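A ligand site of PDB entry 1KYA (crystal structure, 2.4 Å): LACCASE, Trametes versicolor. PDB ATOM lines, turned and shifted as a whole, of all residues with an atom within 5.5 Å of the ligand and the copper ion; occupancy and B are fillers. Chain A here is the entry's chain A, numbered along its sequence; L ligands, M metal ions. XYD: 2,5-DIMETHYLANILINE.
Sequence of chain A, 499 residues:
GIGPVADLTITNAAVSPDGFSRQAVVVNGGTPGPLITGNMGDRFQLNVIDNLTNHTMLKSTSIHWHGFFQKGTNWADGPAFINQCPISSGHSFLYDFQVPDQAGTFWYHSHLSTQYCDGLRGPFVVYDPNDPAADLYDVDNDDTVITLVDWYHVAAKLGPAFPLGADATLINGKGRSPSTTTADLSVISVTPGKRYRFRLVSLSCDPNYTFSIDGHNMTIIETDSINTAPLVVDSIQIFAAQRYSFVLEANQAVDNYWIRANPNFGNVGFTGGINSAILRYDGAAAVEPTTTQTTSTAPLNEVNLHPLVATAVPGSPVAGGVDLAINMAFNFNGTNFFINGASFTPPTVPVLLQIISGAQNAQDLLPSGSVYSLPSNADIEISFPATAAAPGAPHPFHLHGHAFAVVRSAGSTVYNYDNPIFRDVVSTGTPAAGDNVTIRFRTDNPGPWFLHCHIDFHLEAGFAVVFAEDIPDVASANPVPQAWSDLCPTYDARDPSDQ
N of Ile 455 lies close to SG of Cys 453 (3.5 Å).
N of Cys 453 lies within hydrogen-bond range of O of Phe 463 (3.3 Å).
O of Pro 396 sits close to SG of Cys 453, 3.7 Å away.
The backbone carbonyl oxygen (O) of His 458 lies within hydrogen-bond range of the backbone NH (N) of Phe 463.
The copper ion is bound by SG of Cys 453, ND1 of His 458 and ND1 of His 395.
A ring nitrogen (NE2) of His 458 sits at hydrogen-bond distance from a nitrogen (N) of the ligand, 2.6 Å away.
N of the ligand sits at hydrogen-bond distance from OD2 of Asp 206.
Residues that only touch the copper ion: Ile 455 (3.5 Å) and Phe 463 (3.7 Å).
The nearest printed residue that does not touch the copper ion is Pro 396 (4.5 Å).
CD2 of Phe 162 touches C8 of the ligand (3.7 Å).
CD1 of Leu 164 touches C9 of the ligand (3.5 Å).
Phe 265 touches the ligand.
Phe 332 touches the ligand.
Pro 391 touches the ligand.
CA of Gly 392 touches C1 of the ligand (3.8 Å).
Hydrophobic or aromatic side chains within 4 Å of the ligand: Phe 162, Leu 164, Phe 265, Phe 332, Pro 391 and His 458.
Eight residues have an atom within 4 Å of the ligand: Phe 162, Leu 164, Asp 206, Phe 265, Phe 332, Pro 391, Gly 392 and His 458.
Along chain A the residues within 4 Å of the ligand span positions 162 to 458.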
ATOM      1  N   PHE A 162      19.866 -18.587   4.413  1.00  0.00           N
ATOM      2  CA  PHE A 162      19.220 -19.641   3.634  1.00  0.00           C
ATOM      3  C   PHE A 162      18.494 -18.992   2.459  1.00  0.00           C
ATOM      4  O   PHE A 162      17.303 -18.701   2.548  1.00  0.00           O
ATOM      5  CB  PHE A 162      18.226 -20.412   4.515  1.00  0.00           C
ATOM      6  CG  PHE A 162      18.834 -20.966   5.781  1.00  0.00           C
ATOM      7  CD1 PHE A 162      19.892 -21.862   5.722  1.00  0.00           C
ATOM      8  CD2 PHE A 162      18.339 -20.587   7.021  1.00  0.00           C
ATOM      9  CE1 PHE A 162      20.473 -22.384   6.896  1.00  0.00           C
ATOM     10  CE2 PHE A 162      18.905 -21.107   8.212  1.00  0.00           C
ATOM     11  CZ  PHE A 162      19.975 -22.014   8.135  1.00  0.00           C
ATOM     12  N   LEU A 164      16.992 -19.740  -0.440  1.00  0.00           N
ATOM     13  CA  LEU A 164      15.658 -20.143  -0.892  1.00  0.00           C
ATOM     14  C   LEU A 164      15.478 -19.905  -2.408  1.00  0.00           C
ATOM     15  O   LEU A 164      14.417 -19.484  -2.872  1.00  0.00           O
ATOM     16  CB  LEU A 164      14.583 -19.362  -0.109  1.00  0.00           C
ATOM     17  CG  LEU A 164      13.155 -19.898  -0.086  1.00  0.00           C
ATOM     18  CD1 LEU A 164      13.119 -21.235   0.653  1.00  0.00           C
ATOM     19  CD2 LEU A 164      12.250 -18.896   0.617  1.00  0.00           C
ATOM     20  N   ASP A 206      22.562 -25.935  -3.025  1.00  0.00           N
ATOM     21  CA  ASP A 206      21.230 -26.101  -2.367  1.00  0.00           C
ATOM     22  C   ASP A 206      20.178 -26.846  -3.234  1.00  0.00           C
ATOM     23  O   ASP A 206      19.633 -27.857  -2.802  1.00  0.00           O
ATOM     24  CB  ASP A 206      20.697 -24.719  -1.953  1.00  0.00           C
ATOM     25  CG  ASP A 206      19.506 -24.757  -1.014  1.00  0.00           C
ATOM     26  OD1 ASP A 206      18.853 -25.825  -0.968  1.00  0.00           O
ATOM     27  OD2 ASP A 206      19.221 -23.749  -0.335  1.00  0.00           O
ATOM     28  N   PHE A 265      13.335 -25.180  -6.307  1.00  0.00           N
ATOM     29  CA  PHE A 265      12.863 -23.882  -5.821  1.00  0.00           C
ATOM     30  C   PHE A 265      13.734 -22.763  -6.364  1.00  0.00           C
ATOM     31  O   PHE A 265      14.845 -23.002  -6.840  1.00  0.00           O
ATOM     32  CB  PHE A 265      12.800 -23.854  -4.282  1.00  0.00           C
ATOM     33  CG  PHE A 265      14.127 -24.018  -3.614  1.00  0.00           C
ATOM     34  CD1 PHE A 265      14.979 -22.935  -3.437  1.00  0.00           C
ATOM     35  CD2 PHE A 265      14.542 -25.266  -3.161  1.00  0.00           C
ATOM     36  CE1 PHE A 265      16.220 -23.099  -2.821  1.00  0.00           C
ATOM     37  CE2 PHE A 265      15.777 -25.430  -2.533  1.00  0.00           C
ATOM     38  CZ  PHE A 265      16.611 -24.348  -2.372  1.00  0.00           C
ATOM     39  N   PHE A 332      16.242 -28.458  14.275  1.00  0.00           N
ATOM     40  CA  PHE A 332      16.481 -27.082  13.865  1.00  0.00           C
ATOM     41  C   PHE A 332      15.816 -26.155  14.869  1.00  0.00           C
ATOM     42  O   PHE A 332      14.684 -26.399  15.297  1.00  0.00           O
ATOM     43  CB  PHE A 332      15.874 -26.888  12.469  1.00  0.00           C
ATOM     44  CG  PHE A 332      16.218 -25.577  11.830  1.00  0.00           C
ATOM     45  CD1 PHE A 332      17.539 -25.281  11.486  1.00  0.00           C
ATOM     46  CD2 PHE A 332      15.231 -24.644  11.562  1.00  0.00           C
ATOM     47  CE1 PHE A 332      17.857 -24.067  10.874  1.00  0.00           C
ATOM     48  CE2 PHE A 332      15.540 -23.427  10.953  1.00  0.00           C
ATOM     49  CZ  PHE A 332      16.858 -23.140  10.607  1.00  0.00           C
ATOM     50  N   PHE A 337      21.271 -25.867  12.592  1.00  0.00           N
ATOM     51  CA  PHE A 337      20.879 -27.267  12.420  1.00  0.00           C
ATOM     52  C   PHE A 337      21.460 -28.168  13.501  1.00  0.00           C
ATOM     53  O   PHE A 337      22.500 -27.858  14.082  1.00  0.00           O
ATOM     54  CB  PHE A 337      21.314 -27.765  11.043  1.00  0.00           C
ATOM     55  CG  PHE A 337      20.327 -27.462   9.963  1.00  0.00           C
ATOM     56  CD1 PHE A 337      19.134 -28.193   9.868  1.00  0.00           C
ATOM     57  CD2 PHE A 337      20.548 -26.425   9.072  1.00  0.00           C
ATOM     58  CE1 PHE A 337      18.193 -27.881   8.899  1.00  0.00           C
ATOM     59  CE2 PHE A 337      19.604 -26.110   8.094  1.00  0.00           C
ATOM     60  CZ  PHE A 337      18.423 -26.847   8.005  1.00  0.00           C
ATOM     61  N   PRO A 391      13.842 -28.134   8.552  1.00  0.00           N
ATOM     62  CA  PRO A 391      13.381 -27.505   7.304  1.00  0.00           C
ATOM     63  C   PRO A 391      14.425 -27.593   6.208  1.00  0.00           C
ATOM     64  O   PRO A 391      15.619 -27.641   6.482  1.00  0.00           O
ATOM     65  CB  PRO A 391      13.134 -26.052   7.726  1.00  0.00           C
ATOM     66  CG  PRO A 391      12.858 -26.148   9.194  1.00  0.00           C
ATOM     67  CD  PRO A 391      13.876 -27.151   9.648  1.00  0.00           C
ATOM     68  N   GLY A 392      13.985 -27.603   4.953  1.00  0.00           N
ATOM     69  CA  GLY A 392      14.915 -27.649   3.850  1.00  0.00           C
ATOM     70  C   GLY A 392      14.977 -28.978   3.119  1.00  0.00           C
ATOM     71  O   GLY A 392      15.788 -29.173   2.206  1.00  0.00           O
ATOM     72  N   PRO A 394      14.236 -31.998   0.565  1.00  0.00           N
ATOM     73  CA  PRO A 394      15.015 -33.177   0.970  1.00  0.00           C
ATOM     74  C   PRO A 394      16.502 -32.859   1.160  1.00  0.00           C
ATOM     75  O   PRO A 394      17.128 -32.209   0.320  1.00  0.00           O
ATOM     76  CB  PRO A 394      14.762 -34.167  -0.175  1.00  0.00           C
ATOM     77  CG  PRO A 394      14.640 -33.262  -1.355  1.00  0.00           C
ATOM     78  CD  PRO A 394      13.779 -32.118  -0.834  1.00  0.00           C
ATOM     79  N   HIS A 395      17.069 -33.336   2.267  1.00  0.00           N
ATOM     80  CA  HIS A 395      18.461 -33.105   2.585  1.00  0.00           C
ATOM     81  C   HIS A 395      19.350 -34.190   2.010  1.00  0.00           C
ATOM     82  O   HIS A 395      19.246 -35.345   2.394  1.00  0.00           O
ATOM     83  CB  HIS A 395      18.668 -33.069   4.104  1.00  0.00           C
ATOM     84  CG  HIS A 395      17.780 -32.096   4.814  1.00  0.00           C
ATOM     85  ND1 HIS A 395      17.978 -30.733   4.764  1.00  0.00           N
ATOM     86  CD2 HIS A 395      16.702 -32.302   5.615  1.00  0.00           C
ATOM     87  CE1 HIS A 395      17.047 -30.132   5.495  1.00  0.00           C
ATOM     88  NE2 HIS A 395      16.273 -31.064   6.023  1.00  0.00           N
ATOM     89  N   PRO A 396      20.239 -33.808   1.085  1.00  0.00           N
ATOM     90  CA  PRO A 396      21.151 -34.781   0.468  1.00  0.00           C
ATOM     91  C   PRO A 396      22.342 -34.977   1.406  1.00  0.00           C
ATOM     92  O   PRO A 396      23.137 -34.071   1.580  1.00  0.00           O
ATOM     93  CB  PRO A 396      21.590 -34.087  -0.832  1.00  0.00           C
ATOM     94  CG  PRO A 396      20.721 -32.778  -0.899  1.00  0.00           C
ATOM     95  CD  PRO A 396      20.433 -32.464   0.523  1.00  0.00           C
ATOM     96  N   PHE A 397      22.453 -36.148   2.019  1.00  0.00           N
ATOM     97  CA  PHE A 397      23.581 -36.368   2.924  1.00  0.00           C
ATOM     98  C   PHE A 397      24.771 -37.031   2.249  1.00  0.00           C
ATOM     99  O   PHE A 397      24.632 -37.903   1.378  1.00  0.00           O
ATOM    100  CB  PHE A 397      23.171 -37.136   4.176  1.00  0.00           C
ATOM    101  CG  PHE A 397      22.921 -36.241   5.367  1.00  0.00           C
ATOM    102  CD1 PHE A 397      21.788 -35.428   5.429  1.00  0.00           C
ATOM    103  CD2 PHE A 397      23.856 -36.163   6.402  1.00  0.00           C
ATOM    104  CE1 PHE A 397      21.590 -34.542   6.502  1.00  0.00           C
ATOM    105  CE2 PHE A 397      23.670 -35.284   7.480  1.00  0.00           C
ATOM    106  CZ  PHE A 397      22.531 -34.464   7.524  1.00  0.00           C
ATOM    107  N   CYS A 453      25.049 -32.712   5.397  1.00  0.00           N
ATOM    108  CA  CYS A 453      24.112 -32.422   4.341  1.00  0.00           C
ATOM    109  C   CYS A 453      24.902 -31.648   3.300  1.00  0.00           C
ATOM    110  O   CYS A 453      25.712 -30.769   3.647  1.00  0.00           O
ATOM    111  CB  CYS A 453      22.969 -31.574   4.871  1.00  0.00           C
ATOM    112  SG  CYS A 453      21.839 -31.156   3.542  1.00  0.00           S
ATOM    113  N   HIS A 454      24.692 -31.931   2.024  1.00  0.00           N
ATOM    114  CA  HIS A 454      25.452 -31.229   1.009  1.00  0.00           C
ATOM    115  C   HIS A 454      24.831 -29.922   0.528  1.00  0.00           C
ATOM    116  O   HIS A 454      25.224 -29.380  -0.504  1.00  0.00           O
ATOM    117  CB  HIS A 454      25.786 -32.126  -0.162  1.00  0.00           C
ATOM    118  CG  HIS A 454      27.090 -31.789  -0.806  1.00  0.00           C
ATOM    119  ND1 HIS A 454      27.336 -30.574  -1.407  1.00  0.00           N
ATOM    120  CD2 HIS A 454      28.249 -32.493  -0.902  1.00  0.00           C
ATOM    121  CE1 HIS A 454      28.572 -30.538  -1.854  1.00  0.00           C
ATOM    122  NE2 HIS A 454      29.150 -31.693  -1.558  1.00  0.00           N
ATOM    123  N   ILE A 455      23.823 -29.464   1.240  1.00  0.00           N
ATOM    124  CA  ILE A 455      23.265 -28.161   0.982  1.00  0.00           C
ATOM    125  C   ILE A 455      24.189 -27.266   1.787  1.00  0.00           C
ATOM    126  O   ILE A 455      24.008 -27.079   2.999  1.00  0.00           O
ATOM    127  CB  ILE A 455      21.801 -28.015   1.460  1.00  0.00           C
ATOM    128  CG1 ILE A 455      20.857 -28.854   0.593  1.00  0.00           C
ATOM    129  CG2 ILE A 455      21.395 -26.553   1.435  1.00  0.00           C
ATOM    130  CD1 ILE A 455      19.407 -28.786   1.018  1.00  0.00           C
ATOM    131  N   HIS A 458      23.289 -25.318   4.827  1.00  0.00           N
ATOM    132  CA  HIS A 458      22.893 -26.082   6.000  1.00  0.00           C
ATOM    133  C   HIS A 458      24.141 -26.597   6.696  1.00  0.00           C
ATOM    134  O   HIS A 458      24.164 -26.715   7.926  1.00  0.00           O
ATOM    135  CB  HIS A 458      22.002 -27.260   5.612  1.00  0.00           C
ATOM    136  CG  HIS A 458      20.742 -26.857   4.900  1.00  0.00           C
ATOM    137  ND1 HIS A 458      19.800 -27.771   4.491  1.00  0.00           N
ATOM    138  CD2 HIS A 458      20.290 -25.636   4.515  1.00  0.00           C
ATOM    139  CE1 HIS A 458      18.813 -27.130   3.874  1.00  0.00           C
ATOM    140  NE2 HIS A 458      19.083 -25.841   3.888  1.00  0.00           N
ATOM    141  N   PHE A 463      24.740 -28.496  10.300  1.00  0.00           N
ATOM    142  CA  PHE A 463      24.091 -29.765   9.974  1.00  0.00           C
ATOM    143  C   PHE A 463      25.126 -30.796   9.542  1.00  0.00           C
ATOM    144  O   PHE A 463      25.101 -31.272   8.417  1.00  0.00           O
ATOM    145  CB  PHE A 463      23.055 -29.524   8.863  1.00  0.00           C
ATOM    146  CG  PHE A 463      21.926 -30.518   8.853  1.00  0.00           C
ATOM    147  CD1 PHE A 463      21.550 -31.186  10.011  1.00  0.00           C
ATOM    148  CD2 PHE A 463      21.193 -30.732   7.688  1.00  0.00           C
ATOM    149  CE1 PHE A 463      20.458 -32.055  10.014  1.00  0.00           C
ATOM    150  CE2 PHE A 463      20.099 -31.598   7.682  1.00  0.00           C
ATOM    151  CZ  PHE A 463      19.735 -32.259   8.839  1.00  0.00           C
HETATM  152  C1  XYD L   1      16.455 -24.333   2.894  1.00  0.00           C
HETATM  153  C2  XYD L   1      15.060 -24.077   2.301  1.00  0.00           C
HETATM  154  C3  XYD L   1      13.956 -23.552   3.264  1.00  0.00           C
HETATM  155  C4  XYD L   1      14.238 -23.304   4.750  1.00  0.00           C
HETATM  156  C5  XYD L   1      15.654 -23.590   5.304  1.00  0.00           C
HETATM  157  C6  XYD L   1      16.778 -24.101   4.383  1.00  0.00           C
HETATM  158  N   XYD L   1      17.462 -24.780   2.141  1.00  0.00           N
HETATM  159  C8  XYD L   1      15.887 -23.340   6.804  1.00  0.00           C
HETATM  160  C9  XYD L   1      14.775 -24.346   0.820  1.00  0.00           C
HETATM  161 CU    CU M   1      20.135 -29.956   4.242  1.00  0.00          CU
